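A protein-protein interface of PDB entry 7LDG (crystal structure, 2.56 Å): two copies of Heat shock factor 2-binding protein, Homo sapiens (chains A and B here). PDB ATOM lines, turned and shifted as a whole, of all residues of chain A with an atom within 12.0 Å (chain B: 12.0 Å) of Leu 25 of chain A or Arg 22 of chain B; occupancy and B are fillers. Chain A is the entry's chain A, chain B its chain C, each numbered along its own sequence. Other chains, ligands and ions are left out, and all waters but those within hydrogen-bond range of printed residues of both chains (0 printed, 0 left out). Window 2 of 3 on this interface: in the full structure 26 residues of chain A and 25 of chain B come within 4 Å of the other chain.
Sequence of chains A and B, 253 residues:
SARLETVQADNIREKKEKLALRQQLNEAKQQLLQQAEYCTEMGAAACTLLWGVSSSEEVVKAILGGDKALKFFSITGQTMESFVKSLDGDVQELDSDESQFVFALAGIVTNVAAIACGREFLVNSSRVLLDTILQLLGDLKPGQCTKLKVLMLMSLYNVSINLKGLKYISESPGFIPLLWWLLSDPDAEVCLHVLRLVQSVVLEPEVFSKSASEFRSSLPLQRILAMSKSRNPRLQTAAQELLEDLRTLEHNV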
ATOM      1  N   GLN A  24      16.236  30.459  11.340  1.00  0.00           N
ATOM      2  CA  GLN A  24      14.889  30.451  11.916  1.00  0.00           C
ATOM      3  C   GLN A  24      14.945  30.089  13.397  1.00  0.00           C
ATOM      4  O   GLN A  24      14.275  30.711  14.221  1.00  0.00           O
ATOM      5  CB  GLN A  24      13.989  29.463  11.164  1.00  0.00           C
ATOM      6  CG  GLN A  24      13.827  29.751   9.675  1.00  0.00           C
ATOM      7  CD  GLN A  24      13.058  28.656   8.953  1.00  0.00           C
ATOM      8  OE1 GLN A  24      13.047  27.500   9.385  1.00  0.00           O
ATOM      9  NE2 GLN A  24      12.405  29.014   7.850  1.00  0.00           N
ATOM     10  N   LEU A  25      15.738  29.058  13.710  1.00  0.00           N
ATOM     11  CA  LEU A  25      15.962  28.674  15.101  1.00  0.00           C
ATOM     12  C   LEU A  25      16.337  29.882  15.951  1.00  0.00           C
ATOM     13  O   LEU A  25      15.744  30.122  17.006  1.00  0.00           O
ATOM     14  CB  LEU A  25      17.055  27.606  15.186  1.00  0.00           C
ATOM     15  CG  LEU A  25      16.663  26.153  14.960  1.00  0.00           C
ATOM     16  CD1 LEU A  25      17.885  25.365  14.497  1.00  0.00           C
ATOM     17  CD2 LEU A  25      16.100  25.583  16.251  1.00  0.00           C
ATOM     18  N   ASN A  26      17.320  30.662  15.497  1.00  0.00           N
ATOM     19  CA  ASN A  26      17.784  31.795  16.292  1.00  0.00           C
ATOM     20  C   ASN A  26      16.684  32.832  16.461  1.00  0.00           C
ATOM     21  O   ASN A  26      16.545  33.422  17.537  1.00  0.00           O
ATOM     22  CB  ASN A  26      19.032  32.409  15.652  1.00  0.00           C
ATOM     23  CG  ASN A  26      20.202  31.449  15.645  1.00  0.00           C
ATOM     24  OD1 ASN A  26      20.397  30.694  16.598  1.00  0.00           O
ATOM     25  ND2 ASN A  26      20.973  31.451  14.560  1.00  0.00           N
ATOM     26  N   GLU A  27      15.881  33.055  15.415  1.00  0.00           N
ATOM     27  CA  GLU A  27      14.773  34.000  15.526  1.00  0.00           C
ATOM     28  C   GLU A  27      13.729  33.517  16.528  1.00  0.00           C
ATOM     29  O   GLU A  27      13.142  34.323  17.260  1.00  0.00           O
ATOM     30  CB  GLU A  27      14.138  34.232  14.156  1.00  0.00           C
ATOM     31  CG  GLU A  27      15.050  34.909  13.149  1.00  0.00           C
ATOM     32  CD  GLU A  27      14.445  34.950  11.759  1.00  0.00           C
ATOM     33  OE1 GLU A  27      13.409  34.283  11.543  1.00  0.00           O
ATOM     34  OE2 GLU A  27      15.006  35.648  10.886  1.00  0.00           O
ATOM     35  N   ALA A  28      13.486  32.205  16.576  1.00  0.00           N
ATOM     36  CA  ALA A  28      12.535  31.670  17.544  1.00  0.00           C
ATOM     37  C   ALA A  28      13.043  31.852  18.969  1.00  0.00           C
ATOM     38  O   ALA A  28      12.310  32.326  19.844  1.00  0.00           O
ATOM     39  CB  ALA A  28      12.254  30.196  17.253  1.00  0.00           C
ATOM     40  N   LYS A  29      14.304  31.488  19.219  1.00  0.00           N
ATOM     41  CA  LYS A  29      14.872  31.682  20.549  1.00  0.00           C
ATOM     42  C   LYS A  29      14.888  33.156  20.932  1.00  0.00           C
ATOM     43  O   LYS A  29      14.709  33.499  22.104  1.00  0.00           O
ATOM     44  CB  LYS A  29      16.290  31.112  20.611  1.00  0.00           C
ATOM     45  CG  LYS A  29      16.415  29.637  20.282  1.00  0.00           C
ATOM     46  CD  LYS A  29      17.880  29.230  20.226  1.00  0.00           C
ATOM     47  CE  LYS A  29      18.048  27.734  20.026  1.00  0.00           C
ATOM     48  NZ  LYS A  29      19.487  27.351  20.007  1.00  0.00           N
ATOM     49  N   GLN A  30      15.100  34.042  19.954  1.00  0.00           N
ATOM     50  CA  GLN A  30      15.258  35.462  20.256  1.00  0.00           C
ATOM     51  C   GLN A  30      13.990  36.045  20.867  1.00  0.00           C
ATOM     52  O   GLN A  30      14.036  36.679  21.929  1.00  0.00           O
ATOM     53  CB  GLN A  30      15.647  36.227  18.992  1.00  0.00           C
ATOM     54  CG  GLN A  30      17.146  36.273  18.740  1.00  0.00           C
ATOM     55  CD  GLN A  30      17.490  37.071  17.503  1.00  0.00           C
ATOM     56  OE1 GLN A  30      16.657  37.234  16.610  1.00  0.00           O
ATOM     57  NE2 GLN A  30      18.716  37.584  17.447  1.00  0.00           N
ATOM     58  N   GLN A  31      12.843  35.837  20.219  1.00  0.00           N
ATOM     59  CA  GLN A  31      11.598  36.374  20.753  1.00  0.00           C
ATOM     60  C   GLN A  31      11.003  35.510  21.860  1.00  0.00           C
ATOM     61  O   GLN A  31      10.079  35.965  22.542  1.00  0.00           O
ATOM     62  CB  GLN A  31      10.574  36.575  19.620  1.00  0.00           C
ATOM     63  CG  GLN A  31      10.396  35.416  18.665  1.00  0.00           C
ATOM     64  CD  GLN A  31       9.206  34.560  19.027  1.00  0.00           C
ATOM     65  OE1 GLN A  31       9.301  33.708  19.902  1.00  0.00           O
ATOM     66  NE2 GLN A  31       8.076  34.787  18.364  1.00  0.00           N
ATOM     67  N   LEU A  32      11.517  34.293  22.069  1.00  0.00           N
ATOM     68  CA  LEU A  32      11.212  33.566  23.298  1.00  0.00           C
ATOM     69  C   LEU A  32      11.778  34.307  24.502  1.00  0.00           C
ATOM     70  O   LEU A  32      11.092  34.491  25.516  1.00  0.00           O
ATOM     71  CB  LEU A  32      11.769  32.142  23.227  1.00  0.00           C
ATOM     72  CG  LEU A  32      11.436  31.190  24.381  1.00  0.00           C
ATOM     73  CD1 LEU A  32       9.939  31.030  24.509  1.00  0.00           C
ATOM     74  CD2 LEU A  32      12.098  29.830  24.193  1.00  0.00           C
ATOM     75  N   LEU A  33      13.037  34.744  24.403  1.00  0.00           N
ATOM     76  CA  LEU A  33      13.613  35.599  25.436  1.00  0.00           C
ATOM     77  C   LEU A  33      12.844  36.908  25.553  1.00  0.00           C
ATOM     78  O   LEU A  33      12.637  37.422  26.661  1.00  0.00           O
ATOM     79  CB  LEU A  33      15.084  35.878  25.128  1.00  0.00           C
ATOM     80  CG  LEU A  33      16.040  34.685  25.089  1.00  0.00           C
ATOM     81  CD1 LEU A  33      17.348  35.066  24.408  1.00  0.00           C
ATOM     82  CD2 LEU A  33      16.295  34.170  26.495  1.00  0.00           C
ATOM     83  N   GLN A  34      12.419  37.466  24.416  1.00  0.00           N
ATOM     84  CA  GLN A  34      11.686  38.726  24.434  1.00  0.00           C
ATOM     85  C   GLN A  34      10.307  38.562  25.064  1.00  0.00           C
ATOM     86  O   GLN A  34       9.794  39.502  25.681  1.00  0.00           O
ATOM     87  CB  GLN A  34      11.567  39.280  23.015  1.00  0.00           C
ATOM     88  CG  GLN A  34      11.016  40.697  22.936  1.00  0.00           C
ATOM     89  CD  GLN A  34      11.897  41.704  23.650  1.00  0.00           C
ATOM     90  OE1 GLN A  34      12.993  42.025  23.192  1.00  0.00           O
ATOM     91  NE2 GLN A  34      11.420  42.210  24.781  1.00  0.00           N
ATOM     92  N   GLN A  35       9.692  37.383  24.926  1.00  0.00           N
ATOM     93  CA  GLN A  35       8.405  37.152  25.574  1.00  0.00           C
ATOM     94  C   GLN A  35       8.558  36.987  27.078  1.00  0.00           C
ATOM     95  O   GLN A  35       7.689  37.427  27.837  1.00  0.00           O
ATOM     96  CB  GLN A  35       7.725  35.926  24.974  1.00  0.00           C
ATOM     97  CG  GLN A  35       7.074  36.195  23.632  1.00  0.00           C
ATOM     98  CD  GLN A  35       6.369  34.983  23.077  1.00  0.00           C
ATOM     99  OE1 GLN A  35       6.003  34.069  23.819  1.00  0.00           O
ATOM    100  NE2 GLN A  35       6.180  34.962  21.761  1.00  0.00           N
ATOM    101  N   ARG B  22      17.296  22.400  12.426  1.00  0.00           N
ATOM    102  CA  ARG B  22      15.870  22.163  12.275  1.00  0.00           C
ATOM    103  C   ARG B  22      15.428  20.986  13.151  1.00  0.00           C
ATOM    104  O   ARG B  22      14.233  20.667  13.246  1.00  0.00           O
ATOM    105  CB  ARG B  22      15.519  21.904  10.809  1.00  0.00           C
ATOM    106  CG  ARG B  22      16.271  22.784   9.819  1.00  0.00           C
ATOM    107  CD  ARG B  22      16.137  24.271  10.133  1.00  0.00           C
ATOM    108  NE  ARG B  22      17.327  24.815  10.784  1.00  0.00           N
ATOM    109  CZ  ARG B  22      17.623  26.111  10.825  1.00  0.00           C
ATOM    110  NH1 ARG B  22      16.818  26.991  10.242  1.00  0.00           N
ATOM    111  NH2 ARG B  22      18.725  26.534  11.439  1.00  0.00           N
ATOM    112  N   GLN B  23      16.407  20.344  13.780  1.00  0.00           N
ATOM    113  CA  GLN B  23      16.172  19.268  14.727  1.00  0.00           C
ATOM    114  C   GLN B  23      15.993  19.777  16.156  1.00  0.00           C
ATOM    115  O   GLN B  23      16.055  18.981  17.099  1.00  0.00           O
ATOM    116  CB  GLN B  23      17.327  18.259  14.651  1.00  0.00           C
ATOM    117  CG  GLN B  23      17.654  17.856  13.218  1.00  0.00           C
ATOM    118  CD  GLN B  23      18.733  16.792  13.096  1.00  0.00           C
ATOM    119  OE1 GLN B  23      19.760  16.837  13.776  1.00  0.00           O
ATOM    120  NE2 GLN B  23      18.507  15.831  12.203  1.00  0.00           N
ATOM    121  N   GLN B  24      15.767  21.084  16.325  1.00  0.00           N
ATOM    122  CA  GLN B  24      15.501  21.704  17.618  1.00  0.00           C
ATOM    123  C   GLN B  24      14.496  22.846  17.481  1.00  0.00           C
ATOM    124  O   GLN B  24      14.418  23.706  18.368  1.00  0.00           O
ATOM    125  CB  GLN B  24      16.789  22.232  18.273  1.00  0.00           C
ATOM    126  CG  GLN B  24      17.774  21.160  18.710  1.00  0.00           C
ATOM    127  CD  GLN B  24      19.039  21.747  19.299  1.00  0.00           C
ATOM    128  OE1 GLN B  24      19.266  22.957  19.223  1.00  0.00           O
ATOM    129  NE2 GLN B  24      19.873  20.893  19.894  1.00  0.00           N
ATOM    130  N   LEU B  25      13.743  22.887  16.382  1.00  0.00           N
ATOM    131  CA  LEU B  25      12.926  24.047  16.035  1.00  0.00           C
ATOM    132  C   LEU B  25      11.463  23.868  16.422  1.00  0.00           C
ATOM    133  O   LEU B  25      10.904  24.719  17.122  1.00  0.00           O
ATOM    134  CB  LEU B  25      13.048  24.355  14.535  1.00  0.00           C
ATOM    135  CG  LEU B  25      12.327  25.604  14.023  1.00  0.00           C
ATOM    136  CD1 LEU B  25      12.774  26.838  14.793  1.00  0.00           C
ATOM    137  CD2 LEU B  25      12.568  25.779  12.528  1.00  0.00           C
ATOM    138  N   ASN B  26      10.825  22.785  15.968  1.00  0.00           N
ATOM    139  CA  ASN B  26       9.409  22.603  16.269  1.00  0.00           C
ATOM    140  C   ASN B  26       9.176  22.488  17.771  1.00  0.00           C
ATOM    141  O   ASN B  26       8.182  23.008  18.293  1.00  0.00           O
ATOM    142  CB  ASN B  26       8.858  21.380  15.536  1.00  0.00           C
ATOM    143  CG  ASN B  26       9.067  21.459  14.036  1.00  0.00           C
ATOM    144  OD1 ASN B  26       9.048  22.543  13.455  1.00  0.00           O
ATOM    145  ND2 ASN B  26       9.283  20.306  13.402  1.00  0.00           N
ATOM    146  N   GLU B  27      10.092  21.828  18.487  1.00  0.00           N
ATOM    147  CA  GLU B  27       9.970  21.757  19.938  1.00  0.00           C
ATOM    148  C   GLU B  27      10.072  23.145  20.558  1.00  0.00           C
ATOM    149  O   GLU B  27       9.289  23.498  21.445  1.00  0.00           O
ATOM    150  CB  GLU B  27      11.034  20.822  20.514  1.00  0.00           C
ATOM    151  CG  GLU B  27      10.991  19.408  19.961  1.00  0.00           C
ATOM    152  CD  GLU B  27      12.147  18.566  20.461  1.00  0.00           C
ATOM    153  OE1 GLU B  27      13.117  19.156  20.982  1.00  0.00           O
ATOM    154  OE2 GLU B  27      12.088  17.321  20.341  1.00  0.00           O
ATOM    155  N   ALA B  28      11.022  23.958  20.087  1.00  0.00           N
ATOM    156  CA  ALA B  28      11.148  25.310  20.618  1.00  0.00           C
ATOM    157  C   ALA B  28       9.911  26.143  20.308  1.00  0.00           C
ATOM    158  O   ALA B  28       9.544  27.033  21.087  1.00  0.00           O
ATOM    159  CB  ALA B  28      12.400  25.989  20.064  1.00  0.00           C
ATOM    160  N   LYS B  29       9.248  25.863  19.182  1.00  0.00           N
ATOM    161  CA  LYS B  29       8.061  26.632  18.824  1.00  0.00           C
ATOM    162  C   LYS B  29       6.892  26.311  19.750  1.00  0.00           C
ATOM    163  O   LYS B  29       6.106  27.200  20.096  1.00  0.00           O
ATOM    164  CB  LYS B  29       7.679  26.368  17.370  1.00  0.00           C
ATOM    165  CG  LYS B  29       8.589  27.051  16.364  1.00  0.00           C
ATOM    166  CD  LYS B  29       8.356  26.528  14.953  1.00  0.00           C
ATOM    167  CE  LYS B  29       9.186  27.289  13.932  1.00  0.00           C
ATOM    168  NZ  LYS B  29       9.307  26.521  12.662  1.00  0.00           N
ATOM    169  N   GLN B  30       6.745  25.042  20.151  1.00  0.00           N
ATOM    170  CA  GLN B  30       5.673  24.689  21.075  1.00  0.00           C
ATOM    171  C   GLN B  30       5.921  25.290  22.453  1.00  0.00           C
ATOM    172  O   GLN B  30       4.987  25.768  23.106  1.00  0.00           O
ATOM    173  CB  GLN B  30       5.529  23.172  21.156  1.00  0.00           C
ATOM    174  CG  GLN B  30       4.552  22.720  22.222  1.00  0.00           C
ATOM    175  CD  GLN B  30       3.627  21.626  21.741  1.00  0.00           C
ATOM    176  OE1 GLN B  30       3.510  21.376  20.540  1.00  0.00           O
ATOM    177  NE2 GLN B  30       2.960  20.964  22.678  1.00  0.00           N
ATOM    178  N   GLN B  31       7.178  25.280  22.907  1.00  0.00           N
ATOM    179  CA  GLN B  31       7.523  25.955  24.154  1.00  0.00           C
ATOM    180  C   GLN B  31       7.206  27.441  24.088  1.00  0.00           C
ATOM    181  O   GLN B  31       6.861  28.050  25.107  1.00  0.00           O
ATOM    182  CB  GLN B  31       9.003  25.747  24.472  1.00  0.00           C
ATOM    183  CG  GLN B  31       9.408  24.293  24.603  1.00  0.00           C
ATOM    184  CD  GLN B  31      10.912  24.110  24.619  1.00  0.00           C
ATOM    185  OE1 GLN B  31      11.656  24.927  24.077  1.00  0.00           O
ATOM    186  NE2 GLN B  31      11.369  23.032  25.245  1.00  0.00           N
ATOM    187  N   LEU B  32       7.331  28.040  22.903  1.00  0.00           N
ATOM    188  CA  LEU B  32       6.905  29.421  22.719  1.00  0.00           C
ATOM    189  C   LEU B  32       5.421  29.580  23.018  1.00  0.00           C
ATOM    190  O   LEU B  32       5.006  30.520  23.707  1.00  0.00           O
ATOM    191  CB  LEU B  32       7.204  29.869  21.292  1.00  0.00           C
ATOM    192  CG  LEU B  32       6.820  31.326  21.077  1.00  0.00           C
ATOM    193  CD1 LEU B  32       7.745  32.142  21.934  1.00  0.00           C
ATOM    194  CD2 LEU B  32       6.890  31.729  19.607  1.00  0.00           C
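O of Ala 28 of chain A sits close to OE1 of Gln 31 of chain A (3.3 Å).
Among the printed residues, merely in contact across the chains: Gln 24 of chain A with Arg 22 of chain B (3.7 Å), Gln 24 of chain A with Leu 25 of chain B (3.6 Å), Leu 25 of chain A with Arg 22 of chain B (3.4 Å), Leu 25 of chain A with Gln 24 of chain B (3.3 Å), Leu 25 of chain A with Leu 25 of chain B (3.5 Å), Gln 31 of chain A with Leu 32 of chain B (3.0 Å), Leu 32 of chain A with Leu 32 of chain B (3.6 Å) and Gln 35 of chain A with Leu 32 of chain B (3.2 Å).
Of chain B, only Arg 22, Gln 24 and Leu 25 come within 4 Å of Leu 25 of chain A.
Arg 22 of chain B touches two residues of chain A.
Of chain B, only Arg 22 (3.7 Å) and Leu 25 (3.6 Å) come within 4 Å of Gln 24 of chain A.
Asn 26 of chain A touches none of the printed residues of chain B.
No residue of chain B comes within 4 Å of Glu 27 of chain A.
No residue of chain B comes within 4 Å of Lys 29 of chain A.
No residue of chain A comes within 4 Å of Gln 23 of chain B.
Of chain A, only Gln 24 and Leu 25 come within 4 Å of Leu 25 of chain B.
Of the printed residues of chain A, Leu 32 of chain B touches Gln 31, Leu 32 and Gln 35.
Of the printed residues of chain B, Leu 32 of chain A touches Leu 32 (3.6 Å).
Printed residues of chain B within 4 Å of Gln 35 of chain A: Leu 32 (3.2 Å).
The nearest residue of chain B that does not touch Leu 25 of chain A is Gln 23 of chain B (5.3 Å).
Of the 12 printed residues of chain A, 5 touch a printed residue of chain B.
Among the printed residues, 8 pairs touch across the chains.
Gln 24 of chain A touches Leu 25 of chain B, and with the chains exchanged Leu 25 of chain A touches Gln 24 of chain B.
Leu 25 of chain B touches its own counterpart, Leu 25 of chain A.
Gln 31 of chain A touches Leu 32 of chain B, but with the chains exchanged Leu 32 of chain A does not touch Gln 31 of chain B (4.3 Å).
Leu 32 of chain A touches its own counterpart, Leu 32 of chain B.
Of the 8 pairs that touch across the chains among the printed residues, 4 have their exchanged pair printed and touching as well.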
